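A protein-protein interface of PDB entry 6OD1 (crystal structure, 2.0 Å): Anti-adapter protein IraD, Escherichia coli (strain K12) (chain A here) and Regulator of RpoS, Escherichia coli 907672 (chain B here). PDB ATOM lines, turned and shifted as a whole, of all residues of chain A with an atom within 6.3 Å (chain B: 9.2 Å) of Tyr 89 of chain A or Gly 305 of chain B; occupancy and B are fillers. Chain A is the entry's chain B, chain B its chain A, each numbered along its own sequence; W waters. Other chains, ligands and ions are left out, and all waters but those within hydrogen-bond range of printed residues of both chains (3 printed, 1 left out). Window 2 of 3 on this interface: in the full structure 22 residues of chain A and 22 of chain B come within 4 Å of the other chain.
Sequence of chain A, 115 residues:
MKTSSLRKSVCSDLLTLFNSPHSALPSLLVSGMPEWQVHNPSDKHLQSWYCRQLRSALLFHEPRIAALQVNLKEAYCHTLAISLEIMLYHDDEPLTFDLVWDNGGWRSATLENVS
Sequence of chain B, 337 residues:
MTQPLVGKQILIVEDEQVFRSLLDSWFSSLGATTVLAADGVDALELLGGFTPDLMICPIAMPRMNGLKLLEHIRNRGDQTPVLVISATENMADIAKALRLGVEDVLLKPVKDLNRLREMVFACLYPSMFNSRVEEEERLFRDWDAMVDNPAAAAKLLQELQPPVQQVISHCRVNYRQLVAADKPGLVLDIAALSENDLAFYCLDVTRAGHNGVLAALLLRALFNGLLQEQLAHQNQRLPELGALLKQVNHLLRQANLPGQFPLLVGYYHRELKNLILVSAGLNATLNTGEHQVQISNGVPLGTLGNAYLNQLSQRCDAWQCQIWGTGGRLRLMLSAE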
ATOM      1  N   LEU A   6     -34.773 -10.644 -17.243  1.00  0.00           N
ATOM      2  CA  LEU A   6     -34.082  -9.710 -16.361  1.00  0.00           C
ATOM      3  C   LEU A   6     -34.609  -9.804 -14.936  1.00  0.00           C
ATOM      4  O   LEU A   6     -33.830  -9.945 -13.985  1.00  0.00           O
ATOM      5  CB  LEU A   6     -34.229  -8.283 -16.887  1.00  0.00           C
ATOM      6  CG  LEU A   6     -33.889  -7.180 -15.891  1.00  0.00           C
ATOM      7  CD1 LEU A   6     -32.409  -7.241 -15.532  1.00  0.00           C
ATOM      8  CD2 LEU A   6     -34.275  -5.807 -16.443  1.00  0.00           C
ATOM      9  N   PRO A  63     -25.479  -3.735  -9.529  1.00  0.00           N
ATOM     10  CA  PRO A  63     -25.481  -2.558 -10.405  1.00  0.00           C
ATOM     11  C   PRO A  63     -26.754  -2.381 -11.212  1.00  0.00           C
ATOM     12  O   PRO A  63     -26.963  -1.290 -11.765  1.00  0.00           O
ATOM     13  CB  PRO A  63     -24.271  -2.797 -11.324  1.00  0.00           C
ATOM     14  CG  PRO A  63     -23.475  -3.884 -10.669  1.00  0.00           C
ATOM     15  CD  PRO A  63     -24.457  -4.719  -9.920  1.00  0.00           C
ATOM     16  N   ARG A  64     -27.610  -3.404 -11.307  1.00  0.00           N
ATOM     17  CA  ARG A  64     -28.794  -3.334 -12.165  1.00  0.00           C
ATOM     18  C   ARG A  64     -29.966  -2.624 -11.503  1.00  0.00           C
ATOM     19  O   ARG A  64     -30.945  -2.296 -12.186  1.00  0.00           O
ATOM     20  CB  ARG A  64     -29.209  -4.749 -12.585  1.00  0.00           C
ATOM     21  CG  ARG A  64     -28.237  -5.372 -13.570  1.00  0.00           C
ATOM     22  CD  ARG A  64     -28.646  -6.781 -13.950  1.00  0.00           C
ATOM     23  NE  ARG A  64     -28.415  -7.724 -12.866  1.00  0.00           N
ATOM     24  CZ  ARG A  64     -28.729  -9.012 -12.931  1.00  0.00           C
ATOM     25  NH1 ARG A  64     -29.286  -9.499 -14.031  1.00  0.00           N
ATOM     26  NH2 ARG A  64     -28.487  -9.809 -11.904  1.00  0.00           N
ATOM     27  N   ILE A  65     -29.890  -2.400 -10.196  1.00  0.00           N
ATOM     28  CA  ILE A  65     -30.910  -1.666  -9.459  1.00  0.00           C
ATOM     29  C   ILE A  65     -30.651  -0.172  -9.620  1.00  0.00           C
ATOM     30  O   ILE A  65     -29.517   0.299  -9.422  1.00  0.00           O
ATOM     31  CB  ILE A  65     -30.892  -2.080  -7.978  1.00  0.00           C
ATOM     32  CG1 ILE A  65     -31.243  -3.569  -7.826  1.00  0.00           C
ATOM     33  CG2 ILE A  65     -31.787  -1.161  -7.121  1.00  0.00           C
ATOM     34  CD1 ILE A  65     -31.229  -4.049  -6.390  1.00  0.00           C
ATOM     35  N   ALA A  66     -31.699   0.578  -9.977  1.00  0.00           N
ATOM     36  CA  ALA A  66     -31.646   2.036 -10.083  1.00  0.00           C
ATOM     37  C   ALA A  66     -32.194   2.745  -8.854  1.00  0.00           C
ATOM     38  O   ALA A  66     -31.702   3.818  -8.496  1.00  0.00           O
ATOM     39  CB  ALA A  66     -32.422   2.526 -11.319  1.00  0.00           C
ATOM     40  N   ALA A  67     -33.227   2.188  -8.220  1.00  0.00           N
ATOM     41  CA  ALA A  67     -33.781   2.745  -7.000  1.00  0.00           C
ATOM     42  C   ALA A  67     -34.121   1.581  -6.078  1.00  0.00           C
ATOM     43  O   ALA A  67     -34.421   0.479  -6.542  1.00  0.00           O
ATOM     44  CB  ALA A  67     -35.032   3.601  -7.269  1.00  0.00           C
ATOM     45  N   MET A  87     -36.463  -0.626  -8.314  1.00  0.00           N
ATOM     46  CA  MET A  87     -36.607  -0.272  -9.716  1.00  0.00           C
ATOM     47  C   MET A  87     -35.309  -0.594 -10.435  1.00  0.00           C
ATOM     48  O   MET A  87     -34.226  -0.203  -9.982  1.00  0.00           O
ATOM     49  CB  MET A  87     -37.018   1.193  -9.881  1.00  0.00           C
ATOM     50  CG  MET A  87     -38.435   1.374  -9.323  1.00  0.00           C
ATOM     51  SD  MET A  87     -39.646   2.137 -10.403  1.00  0.00           S
ATOM     52  CE  MET A  87     -39.764   0.970 -11.753  1.00  0.00           C
ATOM     53  N   LEU A  88     -35.423  -1.328 -11.538  1.00  0.00           N
ATOM     54  CA  LEU A  88     -34.288  -1.683 -12.380  1.00  0.00           C
ATOM     55  C   LEU A  88     -34.100  -0.668 -13.504  1.00  0.00           C
ATOM     56  O   LEU A  88     -35.067  -0.098 -14.017  1.00  0.00           O
ATOM     57  CB  LEU A  88     -34.498  -3.077 -12.974  1.00  0.00           C
ATOM     58  CG  LEU A  88     -34.777  -4.128 -11.893  1.00  0.00           C
ATOM     59  CD1 LEU A  88     -35.350  -5.415 -12.481  1.00  0.00           C
ATOM     60  CD2 LEU A  88     -33.487  -4.396 -11.138  1.00  0.00           C
ATOM     61  N   TYR A  89     -32.842  -0.441 -13.890  1.00  0.00           N
ATOM     62  CA  TYR A  89     -32.596   0.227 -15.165  1.00  0.00           C
ATOM     63  C   TYR A  89     -33.283  -0.566 -16.266  1.00  0.00           C
ATOM     64  O   TYR A  89     -33.356  -1.801 -16.206  1.00  0.00           O
ATOM     65  CB  TYR A  89     -31.097   0.340 -15.466  1.00  0.00           C
ATOM     66  CG  TYR A  89     -30.342   1.245 -14.511  1.00  0.00           C
ATOM     67  CD1 TYR A  89     -30.415   2.620 -14.622  1.00  0.00           C
ATOM     68  CD2 TYR A  89     -29.584   0.707 -13.480  1.00  0.00           C
ATOM     69  CE1 TYR A  89     -29.730   3.446 -13.744  1.00  0.00           C
ATOM     70  CE2 TYR A  89     -28.899   1.513 -12.600  1.00  0.00           C
ATOM     71  CZ  TYR A  89     -28.983   2.872 -12.721  1.00  0.00           C
ATOM     72  OH  TYR A  89     -28.297   3.667 -11.830  1.00  0.00           O
ATOM     73  N   HIS A  90     -33.845   0.155 -17.233  1.00  0.00           N
ATOM     74  CA  HIS A  90     -34.399  -0.398 -18.464  1.00  0.00           C
ATOM     75  C   HIS A  90     -35.623  -1.288 -18.243  1.00  0.00           C
ATOM     76  O   HIS A  90     -35.975  -2.083 -19.122  1.00  0.00           O
ATOM     77  CB  HIS A  90     -33.319  -1.159 -19.237  1.00  0.00           C
ATOM     78  CG  HIS A  90     -32.029  -0.404 -19.329  1.00  0.00           C
ATOM     79  ND1 HIS A  90     -30.851  -0.868 -18.781  1.00  0.00           N
ATOM     80  CD2 HIS A  90     -31.745   0.807 -19.864  1.00  0.00           C
ATOM     81  CE1 HIS A  90     -29.892   0.018 -18.994  1.00  0.00           C
ATOM     82  NE2 HIS A  90     -30.408   1.040 -19.652  1.00  0.00           N
ATOM     83  N   ASP A  91     -36.297  -1.161 -17.103  1.00  0.00           N
ATOM     84  CA  ASP A  91     -37.571  -1.840 -16.869  1.00  0.00           C
ATOM     85  C   ASP A  91     -38.522  -0.846 -16.223  1.00  0.00           C
ATOM     86  O   ASP A  91     -38.251  -0.347 -15.124  1.00  0.00           O
ATOM     87  CB  ASP A  91     -37.400  -3.079 -15.986  1.00  0.00           C
ATOM     88  CG  ASP A  91     -38.606  -4.021 -16.050  1.00  0.00           C
ATOM     89  OD1 ASP A  91     -38.406  -5.255 -15.968  1.00  0.00           O
ATOM     90  OD2 ASP A  91     -39.748  -3.526 -16.190  1.00  0.00           O
ATOM     91  N   LEU B 245     -20.020  13.138 -14.929  1.00  0.00           N
ATOM     92  CA  LEU B 245     -21.372  12.626 -15.147  1.00  0.00           C
ATOM     93  C   LEU B 245     -21.553  11.272 -14.486  1.00  0.00           C
ATOM     94  O   LEU B 245     -22.603  10.992 -13.896  1.00  0.00           O
ATOM     95  CB  LEU B 245     -21.675  12.508 -16.639  1.00  0.00           C
ATOM     96  CG  LEU B 245     -21.821  13.762 -17.518  1.00  0.00           C
ATOM     97  CD1 LEU B 245     -22.093  13.309 -18.963  1.00  0.00           C
ATOM     98  CD2 LEU B 245     -22.963  14.634 -17.005  1.00  0.00           C
ATOM     99  N   LYS B 246     -20.531  10.415 -14.570  1.00  0.00           N
ATOM    100  CA  LYS B 246     -20.617   9.090 -13.975  1.00  0.00           C
ATOM    101  C   LYS B 246     -20.786   9.181 -12.468  1.00  0.00           C
ATOM    102  O   LYS B 246     -21.569   8.426 -11.860  1.00  0.00           O
ATOM    103  CB  LYS B 246     -19.360   8.305 -14.340  1.00  0.00           C
ATOM    104  CG  LYS B 246     -19.356   6.858 -13.883  1.00  0.00           C
ATOM    105  CD  LYS B 246     -18.083   6.169 -14.368  1.00  0.00           C
ATOM    106  CE  LYS B 246     -17.838   4.889 -13.610  1.00  0.00           C
ATOM    107  NZ  LYS B 246     -16.671   4.174 -14.177  1.00  0.00           N
ATOM    108  N   GLN B 247     -20.074  10.124 -11.853  1.00  0.00           N
ATOM    109  CA  GLN B 247     -20.098  10.279 -10.405  1.00  0.00           C
ATOM    110  C   GLN B 247     -21.389  10.933  -9.933  1.00  0.00           C
ATOM    111  O   GLN B 247     -21.961  10.530  -8.915  1.00  0.00           O
ATOM    112  CB  GLN B 247     -18.864  11.082  -9.971  1.00  0.00           C
ATOM    113  CG  GLN B 247     -17.566  10.279 -10.170  1.00  0.00           C
ATOM    114  CD  GLN B 247     -16.296  11.126 -10.248  1.00  0.00           C
ATOM    115  OE1 GLN B 247     -16.200  12.194  -9.629  1.00  0.00           O
ATOM    116  NE2 GLN B 247     -15.302  10.636 -11.006  1.00  0.00           N
ATOM    117  N   VAL B 248     -21.869  11.944 -10.660  1.00  0.00           N
ATOM    118  CA  VAL B 248     -23.151  12.556 -10.321  1.00  0.00           C
ATOM    119  C   VAL B 248     -24.268  11.524 -10.393  1.00  0.00           C
ATOM    120  O   VAL B 248     -25.183  11.511  -9.558  1.00  0.00           O
ATOM    121  CB  VAL B 248     -23.428  13.751 -11.249  1.00  0.00           C
ATOM    122  CG1 VAL B 248     -24.909  14.198 -11.164  1.00  0.00           C
ATOM    123  CG2 VAL B 248     -22.487  14.887 -10.913  1.00  0.00           C
ATOM    124  N   ASN B 249     -24.211  10.629 -11.381  1.00  0.00           N
ATOM    125  CA  ASN B 249     -25.246   9.593 -11.477  1.00  0.00           C
ATOM    126  C   ASN B 249     -25.205   8.656 -10.270  1.00  0.00           C
ATOM    127  O   ASN B 249     -26.242   8.365  -9.651  1.00  0.00           O
ATOM    128  CB  ASN B 249     -25.080   8.837 -12.801  1.00  0.00           C
ATOM    129  CG  ASN B 249     -26.196   7.841 -13.051  1.00  0.00           C
ATOM    130  OD1 ASN B 249     -27.381   8.189 -13.004  1.00  0.00           O
ATOM    131  ND2 ASN B 249     -25.821   6.588 -13.291  1.00  0.00           N
ATOM    132  N   HIS B 250     -24.012   8.205  -9.874  1.00  0.00           N
ATOM    133  CA  HIS B 250     -23.948   7.361  -8.679  1.00  0.00           C
ATOM    134  C   HIS B 250     -24.392   8.127  -7.441  1.00  0.00           C
ATOM    135  O   HIS B 250     -24.957   7.537  -6.515  1.00  0.00           O
ATOM    136  CB  HIS B 250     -22.539   6.808  -8.468  1.00  0.00           C
ATOM    137  CG  HIS B 250     -22.112   5.826  -9.509  1.00  0.00           C
ATOM    138  ND1 HIS B 250     -20.813   5.738  -9.962  1.00  0.00           N
ATOM    139  CD2 HIS B 250     -22.812   4.888 -10.185  1.00  0.00           C
ATOM    140  CE1 HIS B 250     -20.731   4.788 -10.877  1.00  0.00           C
ATOM    141  NE2 HIS B 250     -21.930   4.258 -11.031  1.00  0.00           N
ATOM    142  N   LEU B 251     -24.162   9.441  -7.410  1.00  0.00           N
ATOM    143  CA  LEU B 251     -24.536  10.238  -6.243  1.00  0.00           C
ATOM    144  C   LEU B 251     -26.056  10.348  -6.099  1.00  0.00           C
ATOM    145  O   LEU B 251     -26.600  10.161  -5.005  1.00  0.00           O
ATOM    146  CB  LEU B 251     -23.897  11.632  -6.359  1.00  0.00           C
ATOM    147  CG  LEU B 251     -24.041  12.582  -5.174  1.00  0.00           C
ATOM    148  CD1 LEU B 251     -23.361  12.016  -3.952  1.00  0.00           C
ATOM    149  CD2 LEU B 251     -23.433  13.950  -5.543  1.00  0.00           C
ATOM    150  N   LEU B 252     -26.756  10.686  -7.190  1.00  0.00           N
ATOM    151  CA  LEU B 252     -28.217  10.775  -7.147  1.00  0.00           C
ATOM    152  C   LEU B 252     -28.847   9.424  -6.822  1.00  0.00           C
ATOM    153  O   LEU B 252     -29.853   9.356  -6.108  1.00  0.00           O
ATOM    154  CB  LEU B 252     -28.758  11.286  -8.473  1.00  0.00           C
ATOM    155  CG  LEU B 252     -28.241  12.676  -8.874  1.00  0.00           C
ATOM    156  CD1 LEU B 252     -28.892  13.153 -10.152  1.00  0.00           C
ATOM    157  CD2 LEU B 252     -28.515  13.634  -7.718  1.00  0.00           C
ATOM    158  N   ARG B 253     -28.280   8.345  -7.357  1.00  0.00           N
ATOM    159  CA  ARG B 253     -28.789   7.014  -7.054  1.00  0.00           C
ATOM    160  C   ARG B 253     -28.679   6.730  -5.563  1.00  0.00           C
ATOM    161  O   ARG B 253     -29.643   6.281  -4.919  1.00  0.00           O
ATOM    162  CB  ARG B 253     -28.001   5.989  -7.864  1.00  0.00           C
ATOM    163  CG  ARG B 253     -28.359   4.524  -7.641  1.00  0.00           C
ATOM    164  CD  ARG B 253     -27.518   3.731  -8.619  1.00  0.00           C
ATOM    165  NE  ARG B 253     -27.644   2.284  -8.476  1.00  0.00           N
ATOM    166  CZ  ARG B 253     -26.758   1.511  -7.868  1.00  0.00           C
ATOM    167  NH1 ARG B 253     -25.681   2.028  -7.301  1.00  0.00           N
ATOM    168  NH2 ARG B 253     -26.941   0.211  -7.839  1.00  0.00           N
ATOM    169  N   GLN B 254     -27.497   6.989  -4.999  1.00  0.00           N
ATOM    170  CA  GLN B 254     -27.278   6.712  -3.584  1.00  0.00           C
ATOM    171  C   GLN B 254     -28.109   7.634  -2.700  1.00  0.00           C
ATOM    172  O   GLN B 254     -28.533   7.225  -1.619  1.00  0.00           O
ATOM    173  CB  GLN B 254     -25.789   6.837  -3.266  1.00  0.00           C
ATOM    174  CG  GLN B 254     -25.465   6.666  -1.790  1.00  0.00           C
ATOM    175  CD  GLN B 254     -25.632   5.228  -1.313  1.00  0.00           C
ATOM    176  OE1 GLN B 254     -25.188   4.292  -1.969  1.00  0.00           O
ATOM    177  NE2 GLN B 254     -26.270   5.056  -0.162  1.00  0.00           N
ATOM    178  N   LEU B 257     -32.659   9.592  -5.216  1.00  0.00           N
ATOM    179  CA  LEU B 257     -33.302  10.552  -6.111  1.00  0.00           C
ATOM    180  C   LEU B 257     -33.419   9.919  -7.490  1.00  0.00           C
ATOM    181  O   LEU B 257     -32.718  10.321  -8.429  1.00  0.00           O
ATOM    182  CB  LEU B 257     -32.517  11.868  -6.169  1.00  0.00           C
ATOM    183  CG  LEU B 257     -32.673  12.682  -4.884  1.00  0.00           C
ATOM    184  CD1 LEU B 257     -31.904  13.998  -4.954  1.00  0.00           C
ATOM    185  CD2 LEU B 257     -34.151  12.916  -4.604  1.00  0.00           C
ATOM    186  N   PRO B 258     -34.277   8.912  -7.647  1.00  0.00           N
ATOM    187  CA  PRO B 258     -34.442   8.299  -8.968  1.00  0.00           C
ATOM    188  C   PRO B 258     -35.184   9.232  -9.913  1.00  0.00           C
ATOM    189  O   PRO B 258     -35.929  10.120  -9.498  1.00  0.00           O
ATOM    190  CB  PRO B 258     -35.264   7.039  -8.686  1.00  0.00           C
ATOM    191  CG  PRO B 258     -36.064   7.373  -7.426  1.00  0.00           C
ATOM    192  CD  PRO B 258     -35.144   8.289  -6.624  1.00  0.00           C
ATOM    193  N   GLY B 259     -34.990   8.996 -11.202  1.00  0.00           N
ATOM    194  CA  GLY B 259     -35.716   9.701 -12.234  1.00  0.00           C
ATOM    195  C   GLY B 259     -34.817   9.948 -13.426  1.00  0.00           C
ATOM    196  O   GLY B 259     -33.759   9.335 -13.558  1.00  0.00           O
ATOM    197  N   PHE B 261     -32.627  12.868 -15.439  1.00  0.00           N
ATOM    198  CA  PHE B 261     -31.967  14.153 -15.207  1.00  0.00           C
ATOM    199  C   PHE B 261     -31.161  14.566 -16.433  1.00  0.00           C
ATOM    200  O   PHE B 261     -29.969  14.234 -16.544  1.00  0.00           O
ATOM    201  CB  PHE B 261     -31.083  14.066 -13.958  1.00  0.00           C
ATOM    202  CG  PHE B 261     -31.830  13.576 -12.732  1.00  0.00           C
ATOM    203  CD1 PHE B 261     -31.808  12.234 -12.368  1.00  0.00           C
ATOM    204  CD2 PHE B 261     -32.573  14.452 -11.963  1.00  0.00           C
ATOM    205  CE1 PHE B 261     -32.517  11.776 -11.250  1.00  0.00           C
ATOM    206  CE2 PHE B 261     -33.299  14.008 -10.848  1.00  0.00           C
ATOM    207  CZ  PHE B 261     -33.257  12.669 -10.481  1.00  0.00           C
ATOM    208  N   VAL B 299     -30.150  10.789 -23.952  1.00  0.00           N
ATOM    209  CA  VAL B 299     -30.124   9.815 -22.861  1.00  0.00           C
ATOM    210  C   VAL B 299     -29.712  10.531 -21.584  1.00  0.00           C
ATOM    211  O   VAL B 299     -28.520  10.805 -21.371  1.00  0.00           O
ATOM    212  CB  VAL B 299     -29.195   8.632 -23.172  1.00  0.00           C
ATOM    213  CG1 VAL B 299     -29.188   7.612 -21.981  1.00  0.00           C
ATOM    214  CG2 VAL B 299     -29.664   7.939 -24.445  1.00  0.00           C
ATOM    215  N   PRO B 300     -30.663  10.849 -20.716  1.00  0.00           N
ATOM    216  CA  PRO B 300     -30.351  11.628 -19.515  1.00  0.00           C
ATOM    217  C   PRO B 300     -29.743  10.753 -18.429  1.00  0.00           C
ATOM    218  O   PRO B 300     -29.807   9.523 -18.481  1.00  0.00           O
ATOM    219  CB  PRO B 300     -31.720  12.174 -19.090  1.00  0.00           C
ATOM    220  CG  PRO B 300     -32.709  11.203 -19.662  1.00  0.00           C
ATOM    221  CD  PRO B 300     -32.107  10.622 -20.898  1.00  0.00           C
ATOM    222  N   LEU B 301     -29.161  11.416 -17.422  1.00  0.00           N
ATOM    223  CA  LEU B 301     -28.737  10.716 -16.214  1.00  0.00           C
ATOM    224  C   LEU B 301     -29.927  10.059 -15.538  1.00  0.00           C
ATOM    225  O   LEU B 301     -31.079  10.488 -15.681  1.00  0.00           O
ATOM    226  CB  LEU B 301     -28.075  11.666 -15.214  1.00  0.00           C
ATOM    227  CG  LEU B 301     -26.552  11.604 -15.165  1.00  0.00           C
ATOM    228  CD1 LEU B 301     -25.998  11.863 -16.547  1.00  0.00           C
ATOM    229  CD2 LEU B 301     -26.002  12.604 -14.154  1.00  0.00           C
ATOM    230  N   GLY B 302     -29.629   9.013 -14.766  1.00  0.00           N
ATOM    231  CA  GLY B 302     -30.642   8.252 -14.110  1.00  0.00           C
ATOM    232  C   GLY B 302     -31.231   7.133 -14.931  1.00  0.00           C
ATOM    233  O   GLY B 302     -32.071   6.390 -14.408  1.00  0.00           O
ATOM    234  N   THR B 303     -30.819   6.974 -16.193  1.00  0.00           N
ATOM    235  CA  THR B 303     -31.359   5.919 -17.041  1.00  0.00           C
ATOM    236  C   THR B 303     -30.346   4.837 -17.392  1.00  0.00           C
ATOM    237  O   THR B 303     -30.737   3.807 -17.948  1.00  0.00           O
ATOM    238  CB  THR B 303     -31.931   6.516 -18.336  1.00  0.00           C
ATOM    239  OG1 THR B 303     -30.878   7.123 -19.083  1.00  0.00           O
ATOM    240  CG2 THR B 303     -32.979   7.575 -18.028  1.00  0.00           C
ATOM    241  N   LEU B 304     -29.064   5.042 -17.090  1.00  0.00           N
ATOM    242  CA  LEU B 304     -28.004   4.067 -17.333  1.00  0.00           C
ATOM    243  C   LEU B 304     -27.239   3.822 -16.038  1.00  0.00           C
ATOM    244  O   LEU B 304     -27.026   4.754 -15.257  1.00  0.00           O
ATOM    245  CB  LEU B 304     -27.012   4.572 -18.400  1.00  0.00           C
ATOM    246  CG  LEU B 304     -27.525   4.843 -19.813  1.00  0.00           C
ATOM    247  CD1 LEU B 304     -26.399   5.360 -20.717  1.00  0.00           C
ATOM    248  CD2 LEU B 304     -28.126   3.567 -20.369  1.00  0.00           C
ATOM    249  N   GLY B 305     -26.788   2.585 -15.829  1.00  0.00           N
ATOM    250  CA  GLY B 305     -25.871   2.330 -14.724  1.00  0.00           C
ATOM    251  C   GLY B 305     -24.627   3.208 -14.787  1.00  0.00           C
ATOM    252  O   GLY B 305     -24.252   3.847 -13.799  1.00  0.00           O
ATOM    253  N   ASN B 306     -23.981   3.263 -15.953  1.00  0.00           N
ATOM    254  CA  ASN B 306     -22.755   4.041 -16.148  1.00  0.00           C
ATOM    255  C   ASN B 306     -23.057   5.231 -17.058  1.00  0.00           C
ATOM    256  O   ASN B 306     -23.327   5.058 -18.250  1.00  0.00           O
ATOM    257  CB  ASN B 306     -21.641   3.158 -16.718  1.00  0.00           C
ATOM    258  CG  ASN B 306     -20.273   3.879 -16.795  1.00  0.00           C
ATOM    259  OD1 ASN B 306     -20.182   5.103 -16.669  1.00  0.00           O
ATOM    260  ND2 ASN B 306     -19.211   3.105 -16.992  1.00  0.00           N
ATOM    261  N   ALA B 307     -23.002   6.443 -16.498  1.00  0.00           N
ATOM    262  CA  ALA B 307     -23.362   7.652 -17.217  1.00  0.00           C
ATOM    263  C   ALA B 307     -22.168   8.330 -17.875  1.00  0.00           C
ATOM    264  O   ALA B 307     -22.304   9.459 -18.351  1.00  0.00           O
ATOM    265  CB  ALA B 307     -24.067   8.634 -16.271  1.00  0.00           C
ATOM    266  N   TYR B 308     -21.013   7.670 -17.931  1.00  0.00           N
ATOM    267  CA  TYR B 308     -19.837   8.272 -18.554  1.00  0.00           C
ATOM    268  C   TYR B 308     -20.102   8.562 -20.030  1.00  0.00           C
ATOM    269  O   TYR B 308     -20.676   7.733 -20.741  1.00  0.00           O
ATOM    270  CB  TYR B 308     -18.621   7.339 -18.409  1.00  0.00           C
ATOM    271  CG  TYR B 308     -17.368   7.901 -19.039  1.00  0.00           C
ATOM    272  CD1 TYR B 308     -17.095   7.696 -20.390  1.00  0.00           C
ATOM    273  CD2 TYR B 308     -16.462   8.654 -18.294  1.00  0.00           C
ATOM    274  CE1 TYR B 308     -15.956   8.235 -20.992  1.00  0.00           C
ATOM    275  CE2 TYR B 308     -15.303   9.210 -18.901  1.00  0.00           C
ATOM    276  CZ  TYR B 308     -15.063   8.984 -20.244  1.00  0.00           C
ATOM    277  OH  TYR B 308     -13.931   9.507 -20.858  1.00  0.00           O
HETATM  278  O   HOH W   1     -31.924   5.606  -6.295  1.00  0.00           O
HETATM  279  O   HOH W   2     -28.947   6.094 -11.923  1.00  0.00           O
HETATM  280  O   HOH W   3     -25.563   3.517 -11.309  1.00  0.00           O
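Hydrophobic or aromatic side chains of chain A that line the printed part of chain B: Ala 67, Tyr 89 and His 90. Printed residues of chain B that touch a printed residue of chain A: Arg 253, Pro 258, Gly 302, Thr 303, Leu 304 and Gly 305. Hydrophobic or aromatic side chains of chain B within 4 Å of the printed part of chain A: Pro 258 and Leu 304. Along chain B the printed residues that touch a printed residue of chain A span positions 253 to 305. Among the printed residues, 10 pairs touch across the chains. Among the printed residues, no Asp or Glu carboxylate lies within 4 Å of a Lys or Arg side-chain nitrogen of the other chain.
Gly 305 of chain B touches just one residue of chain A: Tyr 89 (3.7 Å). Of the printed residues of chain B, His 90 of chain A touches Thr 303 and Leu 304. Printed residues of chain A within 4 Å of Gly 302 of chain B: Tyr 89. Printed residues of chain A within 4 Å of Thr 303 of chain B: Tyr 89 (3.5 Å) and His 90 (3.3 Å). Of the printed residues of chain B, Ile 65 of chain A touches Arg 253. Arg 64 of chain A touches none of the printed residues of chain B. The nearest residue of chain A that does not touch Gly 305 of chain B is Pro 63 of chain A (4.8 Å). The nearest printed residue of chain A that does not touch Gly 302 of chain B is Ala 66 of chain A (5.0 Å).
Among the printed residues, pairs that only touch across the chains: Ala 66 of chain A with Arg 253 of chain B (3.5 Å), Ala 67 of chain A with Pro 258 of chain B (3.7 Å), Tyr 89 of chain A with Arg 253 of chain B (3.3 Å), Tyr 89 of chain A with Gly 302 of chain B (3.8 Å), Tyr 89 of chain A with Thr 303 of chain B (3.5 Å), Tyr 89 of chain A with Leu 304 of chain B (3.4 Å), Tyr 89 of chain A with Gly 305 of chain B (3.7 Å) and His 90 of chain A with Leu 304 of chain B (3.5 Å).
ND2 of Asn 249 of chain B is in hydrogen-bond range of O of Leu 304 of chain B, at 2.9 Å. O of Gly 305 of chain B is in hydrogen-bond range of ND2 of Asn 249 of chain B (3.2 Å). The backbone carbonyl oxygen of Pro 300 of chain B is in hydrogen-bond range of the side-chain hydroxyl of Thr 303 of chain B (2.7 Å). The backbone NH (N) of Tyr 89 of chain A is in hydrogen-bond range of the backbone carbonyl oxygen (O) of Arg 64 of chain A (3.2 Å). The backbone carbonyl oxygen (O) of Met 87 of chain A is in hydrogen-bond range of the backbone NH (N) of Ala 66 of chain A, 2.6 Å away. The backbone carbonyl oxygen (O) of Ala 67 of chain A lies within hydrogen-bond range of the backbone NH (N) of Met 87 of chain A.
Water W2 lies within hydrogen-bond range of OH of Tyr 89 of chain A (2.5 Å) and OD1 of Asn 249 of chain B (2.8 Å). Water W1 bridges O of Arg 253 of chain B (2.7 Å) and O of Ala 66 of chain A (2.8 Å). Water W3 lies within hydrogen-bond range of the side-chain hydroxyl of Tyr 89 of chain A (2.8 Å) and the backbone carbonyl oxygen of Gly 305 of chain B (2.8 Å).
The guanidinium group (NE) of Arg 253 of chain B is in hydrogen-bond range of the backbone carbonyl oxygen (O) of Ile 65 of chain A. O of Thr 303 of chain B sits at hydrogen-bond distance from NE2 of His 90 of chain A (3.3 Å).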
